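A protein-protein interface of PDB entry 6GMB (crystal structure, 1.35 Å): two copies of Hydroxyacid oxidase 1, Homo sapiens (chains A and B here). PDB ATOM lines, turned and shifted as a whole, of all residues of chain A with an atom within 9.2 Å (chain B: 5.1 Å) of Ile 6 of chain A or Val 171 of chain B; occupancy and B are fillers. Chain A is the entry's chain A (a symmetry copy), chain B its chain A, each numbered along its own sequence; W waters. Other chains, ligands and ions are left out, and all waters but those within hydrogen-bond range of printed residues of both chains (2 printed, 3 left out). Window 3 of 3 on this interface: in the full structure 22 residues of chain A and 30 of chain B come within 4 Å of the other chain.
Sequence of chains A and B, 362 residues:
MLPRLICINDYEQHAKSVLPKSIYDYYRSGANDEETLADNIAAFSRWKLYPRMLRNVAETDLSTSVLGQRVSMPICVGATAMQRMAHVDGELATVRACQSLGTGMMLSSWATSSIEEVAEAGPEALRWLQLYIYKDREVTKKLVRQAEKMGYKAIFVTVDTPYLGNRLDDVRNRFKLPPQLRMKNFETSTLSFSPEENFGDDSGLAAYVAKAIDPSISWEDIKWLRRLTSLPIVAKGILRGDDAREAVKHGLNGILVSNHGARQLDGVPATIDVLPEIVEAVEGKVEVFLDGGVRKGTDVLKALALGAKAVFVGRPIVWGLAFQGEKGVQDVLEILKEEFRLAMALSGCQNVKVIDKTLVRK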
ATOM      1  N   PRO A   3     -27.467   2.413  -8.972  1.00  0.00           N
ATOM      2  CA  PRO A   3     -27.505   2.036 -10.386  1.00  0.00           C
ATOM      3  C   PRO A   3     -28.028   3.165 -11.286  1.00  0.00           C
ATOM      4  O   PRO A   3     -29.083   3.758 -11.019  1.00  0.00           O
ATOM      5  CB  PRO A   3     -28.423   0.808 -10.430  1.00  0.00           C
ATOM      6  CG  PRO A   3     -28.288   0.221  -9.048  1.00  0.00           C
ATOM      7  CD  PRO A   3     -28.171   1.428  -8.135  1.00  0.00           C
ATOM      8  N   ARG A   4     -27.233   3.488 -12.305  1.00  0.00           N
ATOM      9  CA  ARG A   4     -27.641   4.375 -13.385  1.00  0.00           C
ATOM     10  C   ARG A   4     -27.466   3.604 -14.697  1.00  0.00           C
ATOM     11  O   ARG A   4     -26.383   3.542 -15.268  1.00  0.00           O
ATOM     12  CB  ARG A   4     -26.838   5.678 -13.355  1.00  0.00           C
ATOM     13  CG  ARG A   4     -27.244   6.677 -14.431  1.00  0.00           C
ATOM     14  CD  ARG A   4     -28.539   7.404 -14.105  1.00  0.00           C
ATOM     15  NE  ARG A   4     -29.119   8.091 -15.258  1.00  0.00           N
ATOM     16  CZ  ARG A   4     -30.166   7.657 -15.960  1.00  0.00           C
ATOM     17  NH1 ARG A   4     -30.716   6.484 -15.693  1.00  0.00           N
ATOM     18  NH2 ARG A   4     -30.666   8.404 -16.929  1.00  0.00           N
ATOM     19  N   LEU A   5     -28.547   2.954 -15.112  1.00  0.00           N
ATOM     20  CA  LEU A   5     -28.516   1.997 -16.206  1.00  0.00           C
ATOM     21  C   LEU A   5     -29.188   2.640 -17.414  1.00  0.00           C
ATOM     22  O   LEU A   5     -30.361   2.985 -17.347  1.00  0.00           O
ATOM     23  CB  LEU A   5     -29.254   0.724 -15.789  1.00  0.00           C
ATOM     24  CG  LEU A   5     -28.851   0.137 -14.437  1.00  0.00           C
ATOM     25  CD1 LEU A   5     -29.636  -1.128 -14.140  1.00  0.00           C
ATOM     26  CD2 LEU A   5     -27.358  -0.128 -14.349  1.00  0.00           C
ATOM     27  N   ILE A   6     -28.421   2.840 -18.486  1.00  0.00           N
ATOM     28  CA  ILE A   6     -28.890   3.692 -19.588  1.00  0.00           C
ATOM     29  C   ILE A   6     -28.901   2.954 -20.928  1.00  0.00           C
ATOM     30  O   ILE A   6     -29.313   3.519 -21.919  1.00  0.00           O
ATOM     31  CB  ILE A   6     -28.067   4.990 -19.658  1.00  0.00           C
ATOM     32  CG1 ILE A   6     -26.617   4.727 -20.065  1.00  0.00           C
ATOM     33  CG2 ILE A   6     -28.156   5.733 -18.334  1.00  0.00           C
ATOM     34  CD1 ILE A   6     -25.843   5.976 -20.403  1.00  0.00           C
ATOM     35  N   CYS A   7     -28.467   1.698 -20.943  1.00  0.00           N
ATOM     36  CA  CYS A   7     -28.479   0.879 -22.153  1.00  0.00           C
ATOM     37  C   CYS A   7     -28.632  -0.577 -21.717  1.00  0.00           C
ATOM     38  O   CYS A   7     -28.487  -0.896 -20.539  1.00  0.00           O
ATOM     39  CB  CYS A   7     -27.224   1.084 -22.996  1.00  0.00           C
ATOM     40  SG  CYS A   7     -25.710   0.547 -22.162  1.00  0.00           S
ATOM     41  N   ILE A   8     -28.908  -1.459 -22.672  1.00  0.00           N
ATOM     42  CA  ILE A   8     -29.175  -2.843 -22.326  1.00  0.00           C
ATOM     43  C   ILE A   8     -27.939  -3.504 -21.696  1.00  0.00           C
ATOM     44  O   ILE A   8     -28.081  -4.267 -20.739  1.00  0.00           O
ATOM     45  CB  ILE A   8     -29.743  -3.623 -23.530  1.00  0.00           C
ATOM     46  CG1 ILE A   8     -31.258  -3.445 -23.671  1.00  0.00           C
ATOM     47  CG2 ILE A   8     -29.424  -5.103 -23.436  1.00  0.00           C
ATOM     48  CD1 ILE A   8     -31.812  -2.072 -23.430  1.00  0.00           C
ATOM     49  N   ASN A   9     -26.737  -3.179 -22.177  1.00  0.00           N
ATOM     50  CA  ASN A   9     -25.530  -3.782 -21.608  1.00  0.00           C
ATOM     51  C   ASN A   9     -25.407  -3.453 -20.113  1.00  0.00           C
ATOM     52  O   ASN A   9     -24.940  -4.281 -19.332  1.00  0.00           O
ATOM     53  CB  ASN A   9     -24.275  -3.348 -22.367  1.00  0.00           C
ATOM     54  CG  ASN A   9     -24.133  -3.984 -23.734  1.00  0.00           C
ATOM     55  OD1 ASN A   9     -24.763  -4.995 -24.030  1.00  0.00           O
ATOM     56  ND2 ASN A   9     -23.282  -3.400 -24.561  1.00  0.00           N
ATOM     57  N   ASP A  10     -25.822  -2.249 -19.709  1.00  0.00           N
ATOM     58  CA  ASP A  10     -25.781  -1.879 -18.299  1.00  0.00           C
ATOM     59  C   ASP A  10     -26.681  -2.800 -17.466  1.00  0.00           C
ATOM     60  O   ASP A  10     -26.345  -3.151 -16.330  1.00  0.00           O
ATOM     61  CB  ASP A  10     -26.230  -0.436 -18.076  1.00  0.00           C
ATOM     62  CG  ASP A  10     -25.318   0.637 -18.635  1.00  0.00           C
ATOM     63  OD1 ASP A  10     -24.173   0.317 -19.018  1.00  0.00           O
ATOM     64  OD2 ASP A  10     -25.764   1.799 -18.646  1.00  0.00           O
ATOM     65  N   TYR A  11     -27.854  -3.143 -18.009  1.00  0.00           N
ATOM     66  CA  TYR A  11     -28.776  -4.057 -17.314  1.00  0.00           C
ATOM     67  C   TYR A  11     -28.130  -5.439 -17.152  1.00  0.00           C
ATOM     68  O   TYR A  11     -28.273  -6.073 -16.115  1.00  0.00           O
ATOM     69  CB  TYR A  11     -30.141  -4.119 -18.013  1.00  0.00           C
ATOM     70  CG  TYR A  11     -31.028  -2.968 -17.616  1.00  0.00           C
ATOM     71  CD1 TYR A  11     -30.892  -1.722 -18.206  1.00  0.00           C
ATOM     72  CD2 TYR A  11     -31.947  -3.097 -16.585  1.00  0.00           C
ATOM     73  CE1 TYR A  11     -31.661  -0.646 -17.798  1.00  0.00           C
ATOM     74  CE2 TYR A  11     -32.725  -2.030 -16.171  1.00  0.00           C
ATOM     75  CZ  TYR A  11     -32.572  -0.794 -16.768  1.00  0.00           C
ATOM     76  OH  TYR A  11     -33.297   0.290 -16.346  1.00  0.00           O
ATOM     77  N   GLU A  12     -27.412  -5.918 -18.169  1.00  0.00           N
ATOM     78  CA  GLU A  12     -26.750  -7.202 -18.022  1.00  0.00           C
ATOM     79  C   GLU A  12     -25.694  -7.139 -16.912  1.00  0.00           C
ATOM     80  O   GLU A  12     -25.568  -8.064 -16.106  1.00  0.00           O
ATOM     81  CB  GLU A  12     -26.077  -7.664 -19.307  1.00  0.00           C
ATOM     82  CG  GLU A  12     -25.468  -9.030 -19.094  1.00  0.00           C
ATOM     83  CD  GLU A  12     -24.886  -9.717 -20.301  1.00  0.00           C
ATOM     84  OE1 GLU A  12     -24.999  -9.169 -21.402  1.00  0.00           O
ATOM     85  OE2 GLU A  12     -24.320 -10.807 -20.114  1.00  0.00           O
ATOM     86  N   HIS A  14     -25.557  -5.220 -14.343  1.00  0.00           N
ATOM     87  CA  HIS A  14     -26.241  -5.199 -13.062  1.00  0.00           C
ATOM     88  C   HIS A  14     -26.718  -6.607 -12.686  1.00  0.00           C
ATOM     89  O   HIS A  14     -26.553  -7.047 -11.557  1.00  0.00           O
ATOM     90  CB  HIS A  14     -27.411  -4.220 -13.083  1.00  0.00           C
ATOM     91  CG  HIS A  14     -28.089  -4.149 -11.765  1.00  0.00           C
ATOM     92  ND1 HIS A  14     -29.168  -4.934 -11.417  1.00  0.00           N
ATOM     93  CD2 HIS A  14     -27.766  -3.433 -10.672  1.00  0.00           C
ATOM     94  CE1 HIS A  14     -29.494  -4.668 -10.161  1.00  0.00           C
ATOM     95  NE2 HIS A  14     -28.660  -3.748  -9.695  1.00  0.00           N
ATOM     96  N   ARG A 295     -29.892  -5.808 -29.160  1.00  0.00           N
ATOM     97  CA  ARG A 295     -29.515  -5.108 -27.944  1.00  0.00           C
ATOM     98  C   ARG A 295     -29.718  -3.596 -28.056  1.00  0.00           C
ATOM     99  O   ARG A 295     -29.712  -2.920 -27.036  1.00  0.00           O
ATOM    100  CB  ARG A 295     -28.045  -5.350 -27.596  1.00  0.00           C
ATOM    101  CG  ARG A 295     -27.649  -6.808 -27.438  1.00  0.00           C
ATOM    102  CD  ARG A 295     -28.279  -7.502 -26.251  1.00  0.00           C
ATOM    103  NE  ARG A 295     -27.912  -8.912 -26.195  1.00  0.00           N
ATOM    104  CZ  ARG A 295     -28.670  -9.934 -26.577  1.00  0.00           C
ATOM    105  NH1 ARG A 295     -29.866  -9.724 -27.109  1.00  0.00           N
ATOM    106  NH2 ARG A 295     -28.220 -11.173 -26.419  1.00  0.00           N
ATOM    107  N   LYS A 296     -29.850  -3.075 -29.277  1.00  0.00           N
ATOM    108  CA  LYS A 296     -29.816  -1.649 -29.549  1.00  0.00           C
ATOM    109  C   LYS A 296     -30.862  -1.299 -30.601  1.00  0.00           C
ATOM    110  O   LYS A 296     -31.234  -2.122 -31.430  1.00  0.00           O
ATOM    111  CB  LYS A 296     -28.456  -1.229 -30.114  1.00  0.00           C
ATOM    112  CG  LYS A 296     -27.277  -1.467 -29.195  1.00  0.00           C
ATOM    113  CD  LYS A 296     -25.995  -0.971 -29.805  1.00  0.00           C
ATOM    114  CE  LYS A 296     -25.489  -1.799 -30.962  1.00  0.00           C
ATOM    115  NZ  LYS A 296     -24.063  -1.479 -31.218  1.00  0.00           N
ATOM    116  N   PHE A 323     -33.134  -6.525 -12.443  1.00  0.00           N
ATOM    117  CA  PHE A 323     -32.998  -5.188 -11.870  1.00  0.00           C
ATOM    118  C   PHE A 323     -34.199  -4.854 -10.974  1.00  0.00           C
ATOM    119  O   PHE A 323     -34.017  -4.486  -9.819  1.00  0.00           O
ATOM    120  CB  PHE A 323     -32.838  -4.128 -12.960  1.00  0.00           C
ATOM    121  CG  PHE A 323     -32.859  -2.727 -12.416  1.00  0.00           C
ATOM    122  CD1 PHE A 323     -31.852  -2.288 -11.578  1.00  0.00           C
ATOM    123  CD2 PHE A 323     -33.907  -1.868 -12.711  1.00  0.00           C
ATOM    124  CE1 PHE A 323     -31.880  -1.002 -11.062  1.00  0.00           C
ATOM    125  CE2 PHE A 323     -33.934  -0.584 -12.194  1.00  0.00           C
ATOM    126  CZ  PHE A 323     -32.922  -0.158 -11.368  1.00  0.00           C
ATOM    127  N   ASP A 331     -38.406  -0.591 -18.239  1.00  0.00           N
ATOM    128  CA  ASP A 331     -37.217   0.222 -18.529  1.00  0.00           C
ATOM    129  C   ASP A 331     -36.492  -0.286 -19.783  1.00  0.00           C
ATOM    130  O   ASP A 331     -36.111   0.498 -20.652  1.00  0.00           O
ATOM    131  CB  ASP A 331     -36.166   0.144 -17.419  1.00  0.00           C
ATOM    132  CG  ASP A 331     -36.447   0.909 -16.145  1.00  0.00           C
ATOM    133  OD1 ASP A 331     -37.386   1.729 -16.138  1.00  0.00           O
ATOM    134  OD2 ASP A 331     -35.689   0.692 -15.165  1.00  0.00           O
ATOM    135  N   VAL A 332     -36.261  -1.601 -19.847  1.00  0.00           N
ATOM    136  CA  VAL A 332     -35.529  -2.178 -20.970  1.00  0.00           C
ATOM    137  C   VAL A 332     -36.307  -1.940 -22.272  1.00  0.00           C
ATOM    138  O   VAL A 332     -35.723  -1.561 -23.292  1.00  0.00           O
ATOM    139  CB  VAL A 332     -35.225  -3.664 -20.719  1.00  0.00           C
ATOM    140  CG1 VAL A 332     -34.883  -4.411 -21.998  1.00  0.00           C
ATOM    141  CG2 VAL A 332     -34.135  -3.816 -19.669  1.00  0.00           C
ATOM    142  N   GLU A 334     -38.514   0.403 -22.855  1.00  0.00           N
ATOM    143  CA  GLU A 334     -38.517   1.835 -23.166  1.00  0.00           C
ATOM    144  C   GLU A 334     -37.165   2.274 -23.743  1.00  0.00           C
ATOM    145  O   GLU A 334     -37.131   3.131 -24.630  1.00  0.00           O
ATOM    146  CB  GLU A 334     -38.882   2.664 -21.940  1.00  0.00           C
ATOM    147  CG  GLU A 334     -40.351   2.579 -21.559  1.00  0.00           C
ATOM    148  CD  GLU A 334     -40.724   3.319 -20.290  1.00  0.00           C
ATOM    149  OE1 GLU A 334     -39.805   3.753 -19.574  1.00  0.00           O
ATOM    150  OE2 GLU A 334     -41.932   3.431 -20.016  1.00  0.00           O
ATOM    151  N   ILE A 335     -36.058   1.711 -23.248  1.00  0.00           N
ATOM    152  CA  ILE A 335     -34.745   2.035 -23.801  1.00  0.00           C
ATOM    153  C   ILE A 335     -34.696   1.586 -25.265  1.00  0.00           C
ATOM    154  O   ILE A 335     -34.256   2.332 -26.139  1.00  0.00           O
ATOM    155  CB  ILE A 335     -33.612   1.412 -22.971  1.00  0.00           C
ATOM    156  CG1 ILE A 335     -33.457   2.151 -21.640  1.00  0.00           C
ATOM    157  CG2 ILE A 335     -32.306   1.386 -23.752  1.00  0.00           C
ATOM    158  CD1 ILE A 335     -32.652   1.404 -20.611  1.00  0.00           C
ATOM    159  N   LEU A 336     -35.133   0.352 -25.532  1.00  0.00           N
ATOM    160  CA  LEU A 336     -35.112  -0.149 -26.905  1.00  0.00           C
ATOM    161  C   LEU A 336     -36.020   0.713 -27.787  1.00  0.00           C
ATOM    162  O   LEU A 336     -35.656   1.040 -28.916  1.00  0.00           O
ATOM    163  CB  LEU A 336     -35.527  -1.621 -26.933  1.00  0.00           C
ATOM    164  CG  LEU A 336     -34.488  -2.591 -26.385  1.00  0.00           C
ATOM    165  CD1 LEU A 336     -35.107  -3.962 -26.169  1.00  0.00           C
ATOM    166  CD2 LEU A 336     -33.273  -2.696 -27.296  1.00  0.00           C
ATOM    167  N   GLU A 338     -36.867   3.904 -27.419  1.00  0.00           N
ATOM    168  CA  GLU A 338     -36.288   5.224 -27.632  1.00  0.00           C
ATOM    169  C   GLU A 338     -35.062   5.129 -28.543  1.00  0.00           C
ATOM    170  O   GLU A 338     -34.873   5.985 -29.404  1.00  0.00           O
ATOM    171  CB  GLU A 338     -35.936   5.897 -26.304  1.00  0.00           C
ATOM    172  CG  GLU A 338     -35.115   7.175 -26.443  1.00  0.00           C
ATOM    173  CD  GLU A 338     -35.784   8.326 -27.179  1.00  0.00           C
ATOM    174  OE1 GLU A 338     -37.017   8.272 -27.402  1.00  0.00           O
ATOM    175  OE2 GLU A 338     -35.061   9.273 -27.539  1.00  0.00           O
ATOM    176  N   GLU A 339     -34.221   4.104 -28.352  1.00  0.00           N
ATOM    177  CA  GLU A 339     -33.078   3.940 -29.249  1.00  0.00           C
ATOM    178  C   GLU A 339     -33.561   3.705 -30.683  1.00  0.00           C
ATOM    179  O   GLU A 339     -32.966   4.204 -31.644  1.00  0.00           O
ATOM    180  CB  GLU A 339     -32.175   2.778 -28.842  1.00  0.00           C
ATOM    181  CG  GLU A 339     -31.388   2.979 -27.552  1.00  0.00           C
ATOM    182  CD  GLU A 339     -30.233   1.998 -27.420  1.00  0.00           C
ATOM    183  OE1 GLU A 339     -29.885   1.332 -28.439  1.00  0.00           O
ATOM    184  OE2 GLU A 339     -29.670   1.907 -26.314  1.00  0.00           O
ATOM    185  N   LEU A 342     -34.832   7.002 -32.169  1.00  0.00           N
ATOM    186  CA  LEU A 342     -33.728   7.874 -32.557  1.00  0.00           C
ATOM    187  C   LEU A 342     -33.050   7.355 -33.832  1.00  0.00           C
ATOM    188  O   LEU A 342     -32.719   8.136 -34.722  1.00  0.00           O
ATOM    189  CB  LEU A 342     -32.740   8.015 -31.400  1.00  0.00           C
ATOM    190  CG  LEU A 342     -31.553   8.936 -31.675  1.00  0.00           C
ATOM    191  CD1 LEU A 342     -32.018  10.359 -31.965  1.00  0.00           C
ATOM    192  CD2 LEU A 342     -30.603   8.915 -30.499  1.00  0.00           C
ATOM    193  N   ASN B 166     -27.026   9.821 -29.263  1.00  0.00           N
ATOM    194  CA  ASN B 166     -26.985   9.349 -27.886  1.00  0.00           C
ATOM    195  C   ASN B 166     -25.538   9.010 -27.515  1.00  0.00           C
ATOM    196  O   ASN B 166     -25.055   7.934 -27.829  1.00  0.00           O
ATOM    197  CB  ASN B 166     -27.901   8.138 -27.733  1.00  0.00           C
ATOM    198  CG  ASN B 166     -28.051   7.645 -26.316  1.00  0.00           C
ATOM    199  OD1 ASN B 166     -27.927   8.412 -25.362  1.00  0.00           O
ATOM    200  ND2 ASN B 166     -28.345   6.364 -26.187  1.00  0.00           N
ATOM    201  N   ARG B 167     -24.849   9.958 -26.874  1.00  0.00           N
ATOM    202  CA  ARG B 167     -23.469   9.777 -26.429  1.00  0.00           C
ATOM    203  C   ARG B 167     -23.538   9.337 -24.964  1.00  0.00           C
ATOM    204  O   ARG B 167     -23.925  10.116 -24.096  1.00  0.00           O
ATOM    205  CB  ARG B 167     -22.646  11.058 -26.615  1.00  0.00           C
ATOM    206  CG  ARG B 167     -22.547  11.584 -28.044  1.00  0.00           C
ATOM    207  CD  ARG B 167     -23.613  12.614 -28.352  1.00  0.00           C
ATOM    208  NE  ARG B 167     -23.551  13.186 -29.693  1.00  0.00           N
ATOM    209  CZ  ARG B 167     -23.210  14.442 -29.986  1.00  0.00           C
ATOM    210  NH1 ARG B 167     -23.473  14.926 -31.191  1.00  0.00           N
ATOM    211  NH2 ARG B 167     -22.610  15.209 -29.084  1.00  0.00           N
ATOM    212  N   LEU B 168     -23.199   8.071 -24.705  1.00  0.00           N
ATOM    213  CA  LEU B 168     -23.482   7.454 -23.414  1.00  0.00           C
ATOM    214  C   LEU B 168     -22.780   8.195 -22.271  1.00  0.00           C
ATOM    215  O   LEU B 168     -23.390   8.409 -21.230  1.00  0.00           O
ATOM    216  CB  LEU B 168     -23.086   5.976 -23.453  1.00  0.00           C
ATOM    217  CG  LEU B 168     -23.854   5.119 -24.457  1.00  0.00           C
ATOM    218  CD1 LEU B 168     -23.399   3.672 -24.383  1.00  0.00           C
ATOM    219  CD2 LEU B 168     -25.356   5.214 -24.237  1.00  0.00           C
ATOM    220  N   ASP B 169     -21.513   8.584 -22.445  1.00  0.00           N
ATOM    221  CA  ASP B 169     -20.825   9.275 -21.353  1.00  0.00           C
ATOM    222  C   ASP B 169     -21.543  10.580 -20.977  1.00  0.00           C
ATOM    223  O   ASP B 169     -21.574  10.938 -19.801  1.00  0.00           O
ATOM    224  CB  ASP B 169     -19.362   9.568 -21.675  1.00  0.00           C
ATOM    225  CG  ASP B 169     -18.434   8.382 -21.491  1.00  0.00           C
ATOM    226  OD1 ASP B 169     -18.730   7.539 -20.623  1.00  0.00           O
ATOM    227  OD2 ASP B 169     -17.418   8.334 -22.203  1.00  0.00           O
ATOM    228  N   ASP B 170     -22.079  11.313 -21.961  1.00  0.00           N
ATOM    229  CA  ASP B 170     -22.773  12.573 -21.675  1.00  0.00           C
ATOM    230  C   ASP B 170     -24.038  12.330 -20.846  1.00  0.00           C
ATOM    231  O   ASP B 170     -24.407  13.170 -20.016  1.00  0.00           O
ATOM    232  CB  ASP B 170     -23.167  13.306 -22.952  1.00  0.00           C
ATOM    233  CG  ASP B 170     -22.002  13.873 -23.734  1.00  0.00           C
ATOM    234  OD1 ASP B 170     -20.866  13.880 -23.207  1.00  0.00           O
ATOM    235  OD2 ASP B 170     -22.253  14.301 -24.867  1.00  0.00           O
ATOM    236  N   VAL B 171     -24.698  11.191 -21.079  1.00  0.00           N
ATOM    237  CA  VAL B 171     -25.852  10.807 -20.280  1.00  0.00           C
ATOM    238  C   VAL B 171     -25.385  10.473 -18.858  1.00  0.00           C
ATOM    239  O   VAL B 171     -25.945  10.976 -17.882  1.00  0.00           O
ATOM    240  CB  VAL B 171     -26.625   9.647 -20.933  1.00  0.00           C
ATOM    241  CG1 VAL B 171     -27.781   9.171 -20.071  1.00  0.00           C
ATOM    242  CG2 VAL B 171     -27.117  10.032 -22.319  1.00  0.00           C
ATOM    243  N   ARG B 172     -24.339   9.644 -18.748  1.00  0.00           N
ATOM    244  CA  ARG B 172     -23.822   9.239 -17.439  1.00  0.00           C
ATOM    245  C   ARG B 172     -23.377  10.464 -16.637  1.00  0.00           C
ATOM    246  O   ARG B 172     -23.634  10.552 -15.433  1.00  0.00           O
ATOM    247  CB  ARG B 172     -22.655   8.261 -17.578  1.00  0.00           C
ATOM    248  CG  ARG B 172     -23.027   6.947 -18.243  1.00  0.00           C
ATOM    249  CD  ARG B 172     -21.914   5.925 -18.158  1.00  0.00           C
ATOM    250  NE  ARG B 172     -22.055   4.848 -19.126  1.00  0.00           N
ATOM    251  CZ  ARG B 172     -22.916   3.839 -19.019  1.00  0.00           C
ATOM    252  NH1 ARG B 172     -23.725   3.751 -17.976  1.00  0.00           N
ATOM    253  NH2 ARG B 172     -22.957   2.916 -19.963  1.00  0.00           N
ATOM    254  N   ASN B 173     -22.700  11.392 -17.315  1.00  0.00           N
ATOM    255  CA  ASN B 173     -22.097  12.561 -16.682  1.00  0.00           C
ATOM    256  C   ASN B 173     -23.105  13.708 -16.518  1.00  0.00           C
ATOM    257  O   ASN B 173     -22.786  14.708 -15.869  1.00  0.00           O
ATOM    258  CB  ASN B 173     -20.911  13.084 -17.493  1.00  0.00           C
ATOM    259  CG  ASN B 173     -19.763  12.104 -17.612  1.00  0.00           C
ATOM    260  OD1 ASN B 173     -19.588  11.229 -16.764  1.00  0.00           O
ATOM    261  ND2 ASN B 173     -18.977  12.249 -18.668  1.00  0.00           N
ATOM    262  N   ARG B 174     -24.292  13.583 -17.131  1.00  0.00           N
ATOM    263  CA  ARG B 174     -25.304  14.654 -17.175  1.00  0.00           C
ATOM    264  C   ARG B 174     -24.648  15.948 -17.668  1.00  0.00           C
ATOM    265  O   ARG B 174     -24.686  17.001 -17.023  1.00  0.00           O
ATOM    266  CB  ARG B 174     -25.997  14.783 -15.818  1.00  0.00           C
ATOM    267  CG  ARG B 174     -26.817  13.550 -15.473  1.00  0.00           C
ATOM    268  CD  ARG B 174     -27.599  13.689 -14.188  1.00  0.00           C
ATOM    269  NE  ARG B 174     -28.549  12.595 -14.019  1.00  0.00           N
ATOM    270  CZ  ARG B 174     -28.307  11.467 -13.358  1.00  0.00           C
ATOM    271  NH1 ARG B 174     -27.109  11.233 -12.849  1.00  0.00           N
ATOM    272  NH2 ARG B 174     -29.269  10.574 -13.206  1.00  0.00           N
ATOM    273  N   ASP B 201     -32.691  15.253 -16.986  1.00  0.00           N
ATOM    274  CA  ASP B 201     -31.901  14.427 -16.076  1.00  0.00           C
ATOM    275  C   ASP B 201     -30.859  13.578 -16.825  1.00  0.00           C
ATOM    276  O   ASP B 201     -30.138  12.805 -16.191  1.00  0.00           O
ATOM    277  CB  ASP B 201     -32.836  13.536 -15.252  1.00  0.00           C
ATOM    278  CG  ASP B 201     -32.149  12.824 -14.101  1.00  0.00           C
ATOM    279  OD1 ASP B 201     -31.510  13.517 -13.285  1.00  0.00           O
ATOM    280  OD2 ASP B 201     -32.238  11.582 -14.041  1.00  0.00           O
ATOM    281  N   ASP B 202     -30.767  13.718 -18.154  1.00  0.00           N
ATOM    282  CA  ASP B 202     -29.841  12.918 -18.975  1.00  0.00           C
ATOM    283  C   ASP B 202     -28.776  13.873 -19.536  1.00  0.00           C
ATOM    284  O   ASP B 202     -28.257  14.700 -18.797  1.00  0.00           O
ATOM    285  CB  ASP B 202     -30.625  12.087 -19.998  1.00  0.00           C
ATOM    286  CG  ASP B 202     -31.545  11.057 -19.359  1.00  0.00           C
ATOM    287  OD1 ASP B 202     -31.183  10.547 -18.286  1.00  0.00           O
ATOM    288  OD2 ASP B 202     -32.611  10.779 -19.941  1.00  0.00           O
ATOM    289  N   SER B 203     -28.419  13.762 -20.819  1.00  0.00           N
ATOM    290  CA  SER B 203     -27.501  14.745 -21.402  1.00  0.00           C
ATOM    291  C   SER B 203     -28.225  16.082 -21.530  1.00  0.00           C
ATOM    292  O   SER B 203     -29.277  16.151 -22.158  1.00  0.00           O
ATOM    293  CB  SER B 203     -26.976  14.343 -22.739  1.00  0.00           C
ATOM    294  OG  SER B 203     -26.345  15.465 -23.352  1.00  0.00           O
HETATM  295  O   HOH W   1     -24.083   5.031 -15.514  1.00  0.00           O
HETATM  296  O   HOH W   2     -29.654   4.046 -24.646  1.00  0.00           O
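The guanidinium group of Arg 172 of chain B is in salt-bridge range of the side-chain carboxylate of Asp 10 of chain A. NH2 of Arg 4 of chain A lies within salt-bridge range of OD1 of Asp 202 of chain B (2.6 Å). The guanidinium group (NE) of Arg 4 of chain A sits close to the guanidinium group (NH2) of Arg 174 of chain B (3.2 Å).
NE of Arg 174 of chain B lies within salt-bridge range of OD1 of Asp 201 of chain B (3.2 Å). The backbone NH (N) of Ile 6 of chain A lies within hydrogen-bond range of the side-chain carboxylate (OD2) of Asp 10 of chain A (2.9 Å). The side-chain sulfur (SG) of Cys 7 of chain A sits at hydrogen-bond distance from the side-chain carboxylate (OD1) of Asp 10 of chain A (3.5 Å).
Among the printed residues, pairs that only touch across the chains: Arg 4 of chain A with Arg 172 of chain B, Ile 6 of chain A with Leu 168 of chain B, Ile 6 of chain A with Val 171 of chain B, Ile 6 of chain A with Arg 172 of chain B and Leu 342 of chain A with Asn 166 of chain B.
Ile 6 of chain A touches just these residues of chain B: Leu 168, Val 171 and Arg 172. Val 171 of chain B touches one residue of chain A. Arg 172 of chain B touches just these residues of chain A: Arg 4 (3.8 Å), Ile 6 (3.7 Å) and Asp 10 (2.9 Å). Printed residues of chain B within 4 Å of Leu 342 of chain A: Asn 166. Printed residues of chain B within 4 Å of Arg 4 of chain A: Arg 172 (3.8 Å), Arg 174 (3.2 Å) and Asp 202 (2.6 Å). Printed residues of chain A within 4 Å of Arg 174 of chain B: Arg 4. Asn 173 of chain B touches none of the printed residues of chain A. Asn 9 of chain A touches none of the printed residues of chain B. The nearest residue of chain A that does not touch Val 171 of chain B is Arg 4 of chain A (4.3 Å). The nearest printed residue of chain A that does not touch Asp 202 of chain B is Ile 6 of chain A (5.7 Å).
Of the 22 printed residues of chain A, 4 touch a printed residue of chain B. Hydrophobic or aromatic side chains of chain A within 4 Å of the printed part of chain B: Ile 6 and Leu 342. Hydrophobic or aromatic side chains of chain B within 4 Å of the printed part of chain A: Leu 168 and Val 171. Along chain B the printed residues that touch a printed residue of chain A span positions 166 to 202.
No position is printed for both chains.
Water W2 lies within hydrogen-bond range of the side-chain carboxylate (OE2) of Glu 339 of chain A, the backbone carbonyl oxygen (O) of Ile 6 of chain A and the side-chain amide nitrogen (ND2) of Asn 166 of chain B. Water W1 lies within hydrogen-bond range of O of Arg 4 of chain A (2.8 Å) and NH1 of Arg 172 of chain B (2.8 Å).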
